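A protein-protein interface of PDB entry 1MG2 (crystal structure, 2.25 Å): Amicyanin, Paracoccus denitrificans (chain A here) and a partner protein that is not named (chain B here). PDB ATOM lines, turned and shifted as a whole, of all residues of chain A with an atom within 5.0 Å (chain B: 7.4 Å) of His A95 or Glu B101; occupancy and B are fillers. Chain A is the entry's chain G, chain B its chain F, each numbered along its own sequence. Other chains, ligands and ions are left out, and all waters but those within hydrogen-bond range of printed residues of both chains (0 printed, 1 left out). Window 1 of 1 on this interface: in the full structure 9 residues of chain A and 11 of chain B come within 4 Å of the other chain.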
ATOM      1  N   MET A  28      23.240 -12.062  22.018  1.00  0.00           N
ATOM      2  CA  MET A  28      23.718 -12.617  20.759  1.00  0.00           C
ATOM      3  C   MET A  28      24.915 -11.884  20.177  1.00  0.00           C
ATOM      4  O   MET A  28      25.024 -11.725  18.960  1.00  0.00           O
ATOM      5  CB  MET A  28      22.587 -12.624  19.727  1.00  0.00           C
ATOM      6  CG  MET A  28      21.350 -13.389  20.173  1.00  0.00           C
ATOM      7  SD  MET A  28      21.753 -15.045  20.749  1.00  0.00           S
ATOM      8  CE  MET A  28      21.914 -15.905  19.191  1.00  0.00           C
ATOM      9  N   MET A  51      21.387 -18.269  26.727  1.00  0.00           N
ATOM     10  CA  MET A  51      21.763 -18.804  25.422  1.00  0.00           C
ATOM     11  C   MET A  51      23.232 -19.237  25.423  1.00  0.00           C
ATOM     12  O   MET A  51      24.129 -18.414  25.620  1.00  0.00           O
ATOM     13  CB  MET A  51      21.554 -17.737  24.348  1.00  0.00           C
ATOM     14  CG  MET A  51      22.022 -18.138  22.959  1.00  0.00           C
ATOM     15  SD  MET A  51      20.967 -19.371  22.213  1.00  0.00           S
ATOM     16  CE  MET A  51      19.577 -18.344  21.713  1.00  0.00           C
ATOM     17  N   PRO A  52      23.497 -20.537  25.218  1.00  0.00           N
ATOM     18  CA  PRO A  52      24.885 -21.012  25.202  1.00  0.00           C
ATOM     19  C   PRO A  52      25.700 -20.399  24.057  1.00  0.00           C
ATOM     20  O   PRO A  52      25.202 -20.235  22.937  1.00  0.00           O
ATOM     21  CB  PRO A  52      24.731 -22.526  25.047  1.00  0.00           C
ATOM     22  CG  PRO A  52      23.423 -22.802  25.712  1.00  0.00           C
ATOM     23  CD  PRO A  52      22.557 -21.672  25.206  1.00  0.00           C
ATOM     24  N   HIS A  53      26.953 -20.058  24.351  1.00  0.00           N
ATOM     25  CA  HIS A  53      27.856 -19.484  23.359  1.00  0.00           C
ATOM     26  C   HIS A  53      29.247 -20.067  23.594  1.00  0.00           C
ATOM     27  O   HIS A  53      29.529 -20.624  24.657  1.00  0.00           O
ATOM     28  CB  HIS A  53      27.941 -17.959  23.508  1.00  0.00           C
ATOM     29  CG  HIS A  53      26.647 -17.243  23.270  1.00  0.00           C
ATOM     30  ND1 HIS A  53      26.047 -17.110  22.038  1.00  0.00           N
ATOM     31  CD2 HIS A  53      25.843 -16.582  24.143  1.00  0.00           C
ATOM     32  CE1 HIS A  53      24.927 -16.390  22.189  1.00  0.00           C
ATOM     33  NE2 HIS A  53      24.757 -16.045  23.450  1.00  0.00           N
ATOM     34  N   CYS A  92      30.955 -17.803  16.853  1.00  0.00           N
ATOM     35  CA  CYS A  92      30.284 -18.751  17.733  1.00  0.00           C
ATOM     36  C   CYS A  92      29.748 -19.857  16.834  1.00  0.00           C
ATOM     37  O   CYS A  92      28.975 -19.591  15.918  1.00  0.00           O
ATOM     38  CB  CYS A  92      29.140 -18.066  18.477  1.00  0.00           C
ATOM     39  SG  CYS A  92      28.304 -19.146  19.634  1.00  0.00           S
ATOM     40  N   THR A  93      30.160 -21.090  17.108  1.00  0.00           N
ATOM     41  CA  THR A  93      29.780 -22.244  16.299  1.00  0.00           C
ATOM     42  C   THR A  93      28.317 -22.350  15.852  1.00  0.00           C
ATOM     43  O   THR A  93      28.042 -22.503  14.663  1.00  0.00           O
ATOM     44  CB  THR A  93      30.193 -23.562  16.992  1.00  0.00           C
ATOM     45  OG1 THR A  93      31.614 -23.580  17.176  1.00  0.00           O
ATOM     46  CG2 THR A  93      29.793 -24.746  16.142  1.00  0.00           C
ATOM     47  N   PRO A  94      27.363 -22.279  16.790  1.00  0.00           N
ATOM     48  CA  PRO A  94      25.962 -22.380  16.364  1.00  0.00           C
ATOM     49  C   PRO A  94      25.383 -21.063  15.847  1.00  0.00           C
ATOM     50  O   PRO A  94      24.320 -21.037  15.232  1.00  0.00           O
ATOM     51  CB  PRO A  94      25.261 -22.854  17.633  1.00  0.00           C
ATOM     52  CG  PRO A  94      26.049 -22.140  18.716  1.00  0.00           C
ATOM     53  CD  PRO A  94      27.478 -22.356  18.260  1.00  0.00           C
ATOM     54  N   HIS A  95      26.093 -19.971  16.105  1.00  0.00           N
ATOM     55  CA  HIS A  95      25.647 -18.643  15.702  1.00  0.00           C
ATOM     56  C   HIS A  95      26.749 -17.974  14.874  1.00  0.00           C
ATOM     57  O   HIS A  95      27.413 -17.050  15.343  1.00  0.00           O
ATOM     58  CB  HIS A  95      25.348 -17.818  16.960  1.00  0.00           C
ATOM     59  CG  HIS A  95      24.502 -18.538  17.970  1.00  0.00           C
ATOM     60  ND1 HIS A  95      24.650 -18.417  19.334  1.00  0.00           N
ATOM     61  CD2 HIS A  95      23.482 -19.419  17.792  1.00  0.00           C
ATOM     62  CE1 HIS A  95      23.747 -19.213  19.931  1.00  0.00           C
ATOM     63  NE2 HIS A  95      23.011 -19.844  19.038  1.00  0.00           N
ATOM     64  N   PRO A  96      26.952 -18.437  13.626  1.00  0.00           N
ATOM     65  CA  PRO A  96      27.972 -17.911  12.712  1.00  0.00           C
ATOM     66  C   PRO A  96      27.938 -16.398  12.556  1.00  0.00           C
ATOM     67  O   PRO A  96      28.955 -15.792  12.226  1.00  0.00           O
ATOM     68  CB  PRO A  96      27.672 -18.634  11.400  1.00  0.00           C
ATOM     69  CG  PRO A  96      27.086 -19.925  11.853  1.00  0.00           C
ATOM     70  CD  PRO A  96      26.171 -19.500  12.970  1.00  0.00           C
ATOM     71  N   PHE A  97      26.775 -15.795  12.789  1.00  0.00           N
ATOM     72  CA  PHE A  97      26.639 -14.348  12.673  1.00  0.00           C
ATOM     73  C   PHE A  97      27.365 -13.640  13.810  1.00  0.00           C
ATOM     74  O   PHE A  97      27.593 -12.431  13.754  1.00  0.00           O
ATOM     75  CB  PHE A  97      25.162 -13.932  12.663  1.00  0.00           C
ATOM     76  CG  PHE A  97      24.352 -14.523  13.783  1.00  0.00           C
ATOM     77  CD1 PHE A  97      23.840 -15.810  13.682  1.00  0.00           C
ATOM     78  CD2 PHE A  97      24.113 -13.797  14.942  1.00  0.00           C
ATOM     79  CE1 PHE A  97      23.097 -16.369  14.721  1.00  0.00           C
ATOM     80  CE2 PHE A  97      23.371 -14.347  15.988  1.00  0.00           C
ATOM     81  CZ  PHE A  97      22.863 -15.637  15.876  1.00  0.00           C
ATOM     82  N   MET A  98      27.710 -14.392  14.851  1.00  0.00           N
ATOM     83  CA  MET A  98      28.444 -13.827  15.978  1.00  0.00           C
ATOM     84  C   MET A  98      29.924 -13.926  15.649  1.00  0.00           C
ATOM     85  O   MET A  98      30.477 -15.019  15.580  1.00  0.00           O
ATOM     86  CB  MET A  98      28.154 -14.602  17.267  1.00  0.00           C
ATOM     87  CG  MET A  98      26.823 -14.261  17.913  1.00  0.00           C
ATOM     88  SD  MET A  98      26.521 -15.265  19.376  1.00  0.00           S
ATOM     89  CE  MET A  98      27.592 -14.483  20.564  1.00  0.00           C
ATOM     90  N   ALA B  55      27.118 -27.831  20.246  1.00  0.00           N
ATOM     91  CA  ALA B  55      26.205 -26.779  19.825  1.00  0.00           C
ATOM     92  C   ALA B  55      24.789 -27.315  19.630  1.00  0.00           C
ATOM     93  O   ALA B  55      24.568 -28.525  19.626  1.00  0.00           O
ATOM     94  CB  ALA B  55      26.711 -26.146  18.534  1.00  0.00           C
ATOM     95  N   SER B  56      23.831 -26.410  19.475  1.00  0.00           N
ATOM     96  CA  SER B  56      22.451 -26.815  19.272  1.00  0.00           C
ATOM     97  C   SER B  56      21.527 -25.626  19.110  1.00  0.00           C
ATOM     98  O   SER B  56      21.933 -24.475  19.223  1.00  0.00           O
ATOM     99  CB  SER B  56      21.952 -27.636  20.462  1.00  0.00           C
ATOM    100  OG  SER B  56      21.667 -26.793  21.563  1.00  0.00           O
ATOM    101  N   TRQ B  57      20.266 -25.926  18.838  1.00  0.00           N
ATOM    102  CA  TRQ B  57      19.252 -24.903  18.730  1.00  0.00           C
ATOM    103  C   TRQ B  57      18.597 -24.938  20.119  1.00  0.00           C
ATOM    104  O   TRQ B  57      18.715 -25.942  20.839  1.00  0.00           O
ATOM    105  CB  TRQ B  57      18.265 -25.255  17.606  1.00  0.00           C
ATOM    106  CG  TRQ B  57      17.445 -26.506  17.815  1.00  0.00           C
ATOM    107  CD1 TRQ B  57      16.240 -26.574  18.459  1.00  0.00           C
ATOM    108  NE1 TRQ B  57      15.776 -27.859  18.474  1.00  0.00           N
ATOM    109  CE2 TRQ B  57      16.681 -28.669  17.838  1.00  0.00           C
ATOM    110  CZ2 TRQ B  57      16.628 -30.052  17.622  1.00  0.00           C
ATOM    111  CH2 TRQ B  57      17.676 -30.637  16.954  1.00  0.00           C
ATOM    112  CZ3 TRQ B  57      18.765 -29.880  16.492  1.00  0.00           C
ATOM    113  CE3 TRQ B  57      18.828 -28.500  16.702  1.00  0.00           C
ATOM    114  CD2 TRQ B  57      17.765 -27.862  17.397  1.00  0.00           C
ATOM    115  O6  TRQ B  57      17.687 -31.854  16.767  1.00  0.00           O
ATOM    116  O7  TRQ B  57      15.651 -30.695  18.038  1.00  0.00           O
ATOM    117  N   VAL B  58      17.941 -23.856  20.520  1.00  0.00           N
ATOM    118  CA  VAL B  58      17.312 -23.833  21.833  1.00  0.00           C
ATOM    119  C   VAL B  58      15.856 -23.402  21.769  1.00  0.00           C
ATOM    120  O   VAL B  58      15.345 -23.037  20.711  1.00  0.00           O
ATOM    121  CB  VAL B  58      18.060 -22.882  22.808  1.00  0.00           C
ATOM    122  CG1 VAL B  58      19.523 -23.267  22.895  1.00  0.00           C
ATOM    123  CG2 VAL B  58      17.914 -21.436  22.359  1.00  0.00           C
ATOM    124  N   ALA B  59      15.196 -23.456  22.917  1.00  0.00           N
ATOM    125  CA  ALA B  59      13.803 -23.062  23.031  1.00  0.00           C
ATOM    126  C   ALA B  59      13.438 -22.950  24.499  1.00  0.00           C
ATOM    127  O   ALA B  59      13.939 -23.701  25.335  1.00  0.00           O
ATOM    128  CB  ALA B  59      12.904 -24.081  22.355  1.00  0.00           C
ATOM    129  N   LEU B  71      15.259 -22.818  29.531  1.00  0.00           N
ATOM    130  CA  LEU B  71      15.868 -22.848  28.213  1.00  0.00           C
ATOM    131  C   LEU B  71      16.429 -24.252  28.008  1.00  0.00           C
ATOM    132  O   LEU B  71      17.286 -24.708  28.772  1.00  0.00           O
ATOM    133  CB  LEU B  71      16.994 -21.822  28.111  1.00  0.00           C
ATOM    134  CG  LEU B  71      17.503 -21.594  26.687  1.00  0.00           C
ATOM    135  CD1 LEU B  71      16.376 -20.982  25.845  1.00  0.00           C
ATOM    136  CD2 LEU B  71      18.713 -20.676  26.713  1.00  0.00           C
ATOM    137  N   ILE B  72      15.932 -24.933  26.982  1.00  0.00           N
ATOM    138  CA  ILE B  72      16.371 -26.286  26.667  1.00  0.00           C
ATOM    139  C   ILE B  72      17.361 -26.223  25.510  1.00  0.00           C
ATOM    140  O   ILE B  72      17.090 -25.574  24.503  1.00  0.00           O
ATOM    141  CB  ILE B  72      15.167 -27.175  26.246  1.00  0.00           C
ATOM    142  CG1 ILE B  72      14.096 -27.170  27.341  1.00  0.00           C
ATOM    143  CG2 ILE B  72      15.636 -28.598  25.970  1.00  0.00           C
ATOM    144  CD1 ILE B  72      14.561 -27.731  28.671  1.00  0.00           C
ATOM    145  N   LEU B  95      11.914 -20.680  15.173  1.00  0.00           N
ATOM    146  CA  LEU B  95      12.032 -19.657  14.137  1.00  0.00           C
ATOM    147  C   LEU B  95      12.686 -20.164  12.845  1.00  0.00           C
ATOM    148  O   LEU B  95      13.384 -21.185  12.847  1.00  0.00           O
ATOM    149  CB  LEU B  95      12.829 -18.473  14.693  1.00  0.00           C
ATOM    150  CG  LEU B  95      12.071 -17.344  15.414  1.00  0.00           C
ATOM    151  CD1 LEU B  95      10.917 -17.887  16.228  1.00  0.00           C
ATOM    152  CD2 LEU B  95      13.044 -16.574  16.293  1.00  0.00           C
ATOM    153  N   PRO B  96      12.465 -19.456  11.723  1.00  0.00           N
ATOM    154  CA  PRO B  96      13.049 -19.863  10.437  1.00  0.00           C
ATOM    155  C   PRO B  96      14.569 -19.968  10.491  1.00  0.00           C
ATOM    156  O   PRO B  96      15.199 -19.494  11.434  1.00  0.00           O
ATOM    157  CB  PRO B  96      12.563 -18.782   9.477  1.00  0.00           C
ATOM    158  CG  PRO B  96      11.238 -18.377  10.079  1.00  0.00           C
ATOM    159  CD  PRO B  96      11.575 -18.295  11.551  1.00  0.00           C
ATOM    160  N   VAL B  97      15.155 -20.576   9.465  1.00  0.00           N
ATOM    161  CA  VAL B  97      16.596 -20.788   9.419  1.00  0.00           C
ATOM    162  C   VAL B  97      17.478 -19.534   9.503  1.00  0.00           C
ATOM    163  O   VAL B  97      18.631 -19.623   9.925  1.00  0.00           O
ATOM    164  CB  VAL B  97      16.987 -21.606   8.162  1.00  0.00           C
ATOM    165  CG1 VAL B  97      16.942 -20.718   6.926  1.00  0.00           C
ATOM    166  CG2 VAL B  97      18.368 -22.227   8.348  1.00  0.00           C
ATOM    167  N   TYR B  98      16.962 -18.371   9.110  1.00  0.00           N
ATOM    168  CA  TYR B  98      17.771 -17.156   9.187  1.00  0.00           C
ATOM    169  C   TYR B  98      17.933 -16.666  10.638  1.00  0.00           C
ATOM    170  O   TYR B  98      18.569 -15.640  10.896  1.00  0.00           O
ATOM    171  CB  TYR B  98      17.189 -16.058   8.285  1.00  0.00           C
ATOM    172  CG  TYR B  98      15.799 -15.590   8.626  1.00  0.00           C
ATOM    173  CD1 TYR B  98      15.593 -14.497   9.467  1.00  0.00           C
ATOM    174  CD2 TYR B  98      14.683 -16.222   8.079  1.00  0.00           C
ATOM    175  CE1 TYR B  98      14.304 -14.041   9.752  1.00  0.00           C
ATOM    176  CE2 TYR B  98      13.396 -15.778   8.360  1.00  0.00           C
ATOM    177  CZ  TYR B  98      13.211 -14.689   9.194  1.00  0.00           C
ATOM    178  OH  TYR B  98      11.931 -14.266   9.475  1.00  0.00           O
ATOM    179  N   ARG B  99      17.342 -17.413  11.566  1.00  0.00           N
ATOM    180  CA  ARG B  99      17.442 -17.158  13.006  1.00  0.00           C
ATOM    181  C   ARG B  99      17.818 -18.543  13.559  1.00  0.00           C
ATOM    182  O   ARG B  99      17.109 -19.121  14.390  1.00  0.00           O
ATOM    183  CB  ARG B  99      16.095 -16.710  13.589  1.00  0.00           C
ATOM    184  CG  ARG B  99      15.643 -15.310  13.180  1.00  0.00           C
ATOM    185  CD  ARG B  99      16.579 -14.230  13.715  1.00  0.00           C
ATOM    186  NE  ARG B  99      16.671 -14.217  15.176  1.00  0.00           N
ATOM    187  CZ  ARG B  99      15.709 -13.793  15.994  1.00  0.00           C
ATOM    188  NH1 ARG B  99      15.894 -13.826  17.307  1.00  0.00           N
ATOM    189  NH2 ARG B  99      14.567 -13.327  15.509  1.00  0.00           N
ATOM    190  N   PRO B 100      18.954 -19.087  13.094  1.00  0.00           N
ATOM    191  CA  PRO B 100      19.462 -20.401  13.493  1.00  0.00           C
ATOM    192  C   PRO B 100      19.423 -20.759  14.970  1.00  0.00           C
ATOM    193  O   PRO B 100      19.140 -21.906  15.314  1.00  0.00           O
ATOM    194  CB  PRO B 100      20.882 -20.413  12.922  1.00  0.00           C
ATOM    195  CG  PRO B 100      21.257 -18.972  12.915  1.00  0.00           C
ATOM    196  CD  PRO B 100      20.005 -18.315  12.413  1.00  0.00           C
ATOM    197  N   GLU B 101      19.694 -19.795  15.843  1.00  0.00           N
ATOM    198  CA  GLU B 101      19.687 -20.072  17.279  1.00  0.00           C
ATOM    199  C   GLU B 101      18.379 -20.732  17.748  1.00  0.00           C
ATOM    200  O   GLU B 101      18.360 -21.398  18.781  1.00  0.00           O
ATOM    201  CB  GLU B 101      19.942 -18.790  18.082  1.00  0.00           C
ATOM    202  CG  GLU B 101      18.873 -17.719  17.925  1.00  0.00           C
ATOM    203  CD  GLU B 101      19.148 -16.763  16.774  1.00  0.00           C
ATOM    204  OE1 GLU B 101      19.785 -17.176  15.782  1.00  0.00           O
ATOM    205  OE2 GLU B 101      18.712 -15.597  16.861  1.00  0.00           O
ATOM    206  N   PHE B 102      17.301 -20.561  16.980  1.00  0.00           N
ATOM    207  CA  PHE B 102      15.996 -21.137  17.318  1.00  0.00           C
ATOM    208  C   PHE B 102      15.417 -22.043  16.227  1.00  0.00           C
ATOM    209  O   PHE B 102      14.243 -22.418  16.292  1.00  0.00           O
ATOM    210  CB  PHE B 102      14.974 -20.029  17.597  1.00  0.00           C
ATOM    211  CG  PHE B 102      15.323 -19.142  18.763  1.00  0.00           C
ATOM    212  CD1 PHE B 102      15.417 -19.659  20.051  1.00  0.00           C
ATOM    213  CD2 PHE B 102      15.545 -17.781  18.570  1.00  0.00           C
ATOM    214  CE1 PHE B 102      15.725 -18.835  21.125  1.00  0.00           C
ATOM    215  CE2 PHE B 102      15.854 -16.949  19.643  1.00  0.00           C
ATOM    216  CZ  PHE B 102      15.945 -17.477  20.920  1.00  0.00           C
ATOM    217  N   ALA B 103      16.228 -22.389  15.229  1.00  0.00           N
ATOM    218  CA  ALA B 103      15.773 -23.233  14.123  1.00  0.00           C
ATOM    219  C   ALA B 103      16.050 -24.715  14.378  1.00  0.00           C
ATOM    220  O   ALA B 103      17.187 -25.090  14.684  1.00  0.00           O
ATOM    221  CB  ALA B 103      16.448 -22.785  12.827  1.00  0.00           C
ATOM    222  N   ASN B 104      15.030 -25.563  14.238  1.00  0.00           N
ATOM    223  CA  ASN B 104      15.240 -26.981  14.501  1.00  0.00           C
ATOM    224  C   ASN B 104      15.238 -27.980  13.334  1.00  0.00           C
ATOM    225  O   ASN B 104      15.123 -29.186  13.559  1.00  0.00           O
ATOM    226  CB  ASN B 104      14.299 -27.461  15.630  1.00  0.00           C
ATOM    227  CG  ASN B 104      12.836 -27.576  15.205  1.00  0.00           C
ATOM    228  OD1 ASN B 104      11.961 -27.756  16.055  1.00  0.00           O
ATOM    229  ND2 ASN B 104      12.564 -27.494  13.909  1.00  0.00           N
ATOM    230  N   ILE B 106      17.759 -27.872  11.386  1.00  0.00           N
ATOM    231  CA  ILE B 106      19.208 -27.984  11.291  1.00  0.00           C
ATOM    232  C   ILE B 106      19.717 -29.174  12.087  1.00  0.00           C
ATOM    233  O   ILE B 106      19.250 -29.433  13.195  1.00  0.00           O
ATOM    234  CB  ILE B 106      19.891 -26.713  11.836  1.00  0.00           C
ATOM    235  CG1 ILE B 106      19.494 -25.509  10.983  1.00  0.00           C
ATOM    236  CG2 ILE B 106      21.404 -26.902  11.870  1.00  0.00           C
ATOM    237  CD1 ILE B 106      20.026 -24.186  11.512  1.00  0.00           C
ATOM    238  N   TRP B 108      21.922 -30.386  14.436  1.00  0.00           N
ATOM    239  CA  TRP B 108      22.804 -29.840  15.454  1.00  0.00           C
ATOM    240  C   TRP B 108      23.836 -30.849  15.964  1.00  0.00           C
ATOM    241  O   TRP B 108      23.767 -31.304  17.103  1.00  0.00           O
ATOM    242  CB  TRP B 108      21.951 -29.263  16.599  1.00  0.00           C
ATOM    243  CG  TRP B 108      21.242 -27.986  16.186  1.00  0.00           C
ATOM    244  CD1 TRP B 108      19.879 -27.745  16.132  1.00  0.00           C
ATOM    245  CD2 TRP B 108      21.876 -26.790  15.713  1.00  0.00           C
ATOM    246  NE1 TRP B 108      19.655 -26.482  15.645  1.00  0.00           N
ATOM    247  CE2 TRP B 108      20.856 -25.874  15.387  1.00  0.00           C
ATOM    248  CE3 TRP B 108      23.213 -26.407  15.537  1.00  0.00           C
ATOM    249  CZ2 TRP B 108      21.129 -24.595  14.894  1.00  0.00           C
ATOM    250  CZ3 TRP B 108      23.486 -25.133  15.046  1.00  0.00           C
ATOM    251  CH2 TRP B 108      22.448 -24.244  14.732  1.00  0.00           C
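Of the printed residues of chain B, Pro A94 touches Ala B55 (3.7 Å) and Trp B108 (3.7 Å).
His A95 touches one residue of chain B.
Of the printed residues of chain A, Leu B71 touches Met A51 (3.6 Å).
Ile B72 touches none of the printed residues of chain A.
Glu B101 touches just these residues of chain A: Met A28, Met A51, His A95 and Phe A97.
Ala B103 touches none of the printed residues of chain A.
Of the printed residues of chain A, Trp B108 touches Pro A94.
The nearest residue of chain B that does not touch His A95 is Ser B56 (4.8 Å).
Printed residues of chain B that touch a printed residue of chain A: Ala B55, Val B58, Leu B71, Pro B100, Glu B101, Phe B102 and Trp B108.
Hydrophobic or aromatic side chains of chain B that line the printed part of chain A: Ala B55, Val B58, Leu B71, Pro B100, Phe B102 and Trp B108.
Of the 11 printed residues of chain A, 5 touch a printed residue of chain B.
Hydrophobic or aromatic side chains of chain A within 4 Å of the printed part of chain B: Met A28, Met A51, Pro A94, His A95 and Phe A97.
Among the printed residues, 10 pairs touch across the chains.
The side-chain sulfur (SD) of Met A98 sits close to a ring nitrogen (ND1) of His A95 (3.7 Å).
O of Met A51 lies close to NE2 of His A53, 3.3 Å away.
The guanidinium group (NE) of Arg B99 lies within salt-bridge range of the side-chain carboxylate (OE2) of Glu B101, at 3.0 Å.
The backbone carbonyl oxygen (O) of Ala B103 is in hydrogen-bond range of NE1 of Trp B108 (3.0 Å).
N of Val B58 lies within hydrogen-bond range of O of Glu B101 (3.0 Å).
The backbone carbonyl oxygen (O) of Phe B102 is in hydrogen-bond range of the backbone NH (N) of Leu B95.
Glu B101 touches Met A28 (CB to CE, 3.7 Å).
Met A51 touches Val B58 (CE to CG2, 3.6 Å).
Leu B71 touches Met A51.
Met A51 touches Glu B101 (CE to CB, 3.7 Å).
Met A51 touches Phe B102 (CE to CZ, 3.8 Å).
CB of Ala B55 touches CB of Pro A94, 3.7 Å away.
CH2 of Trp B108 touches O of Pro A94, at 3.7 Å.
NE2 of His A95 touches CB of Glu B101, at 3.4 Å.
CG of Pro B100 touches CE1 of Phe A97 (3.7 Å).
CZ of Phe A97 touches OE1 of Glu B101, 3.4 Å away.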
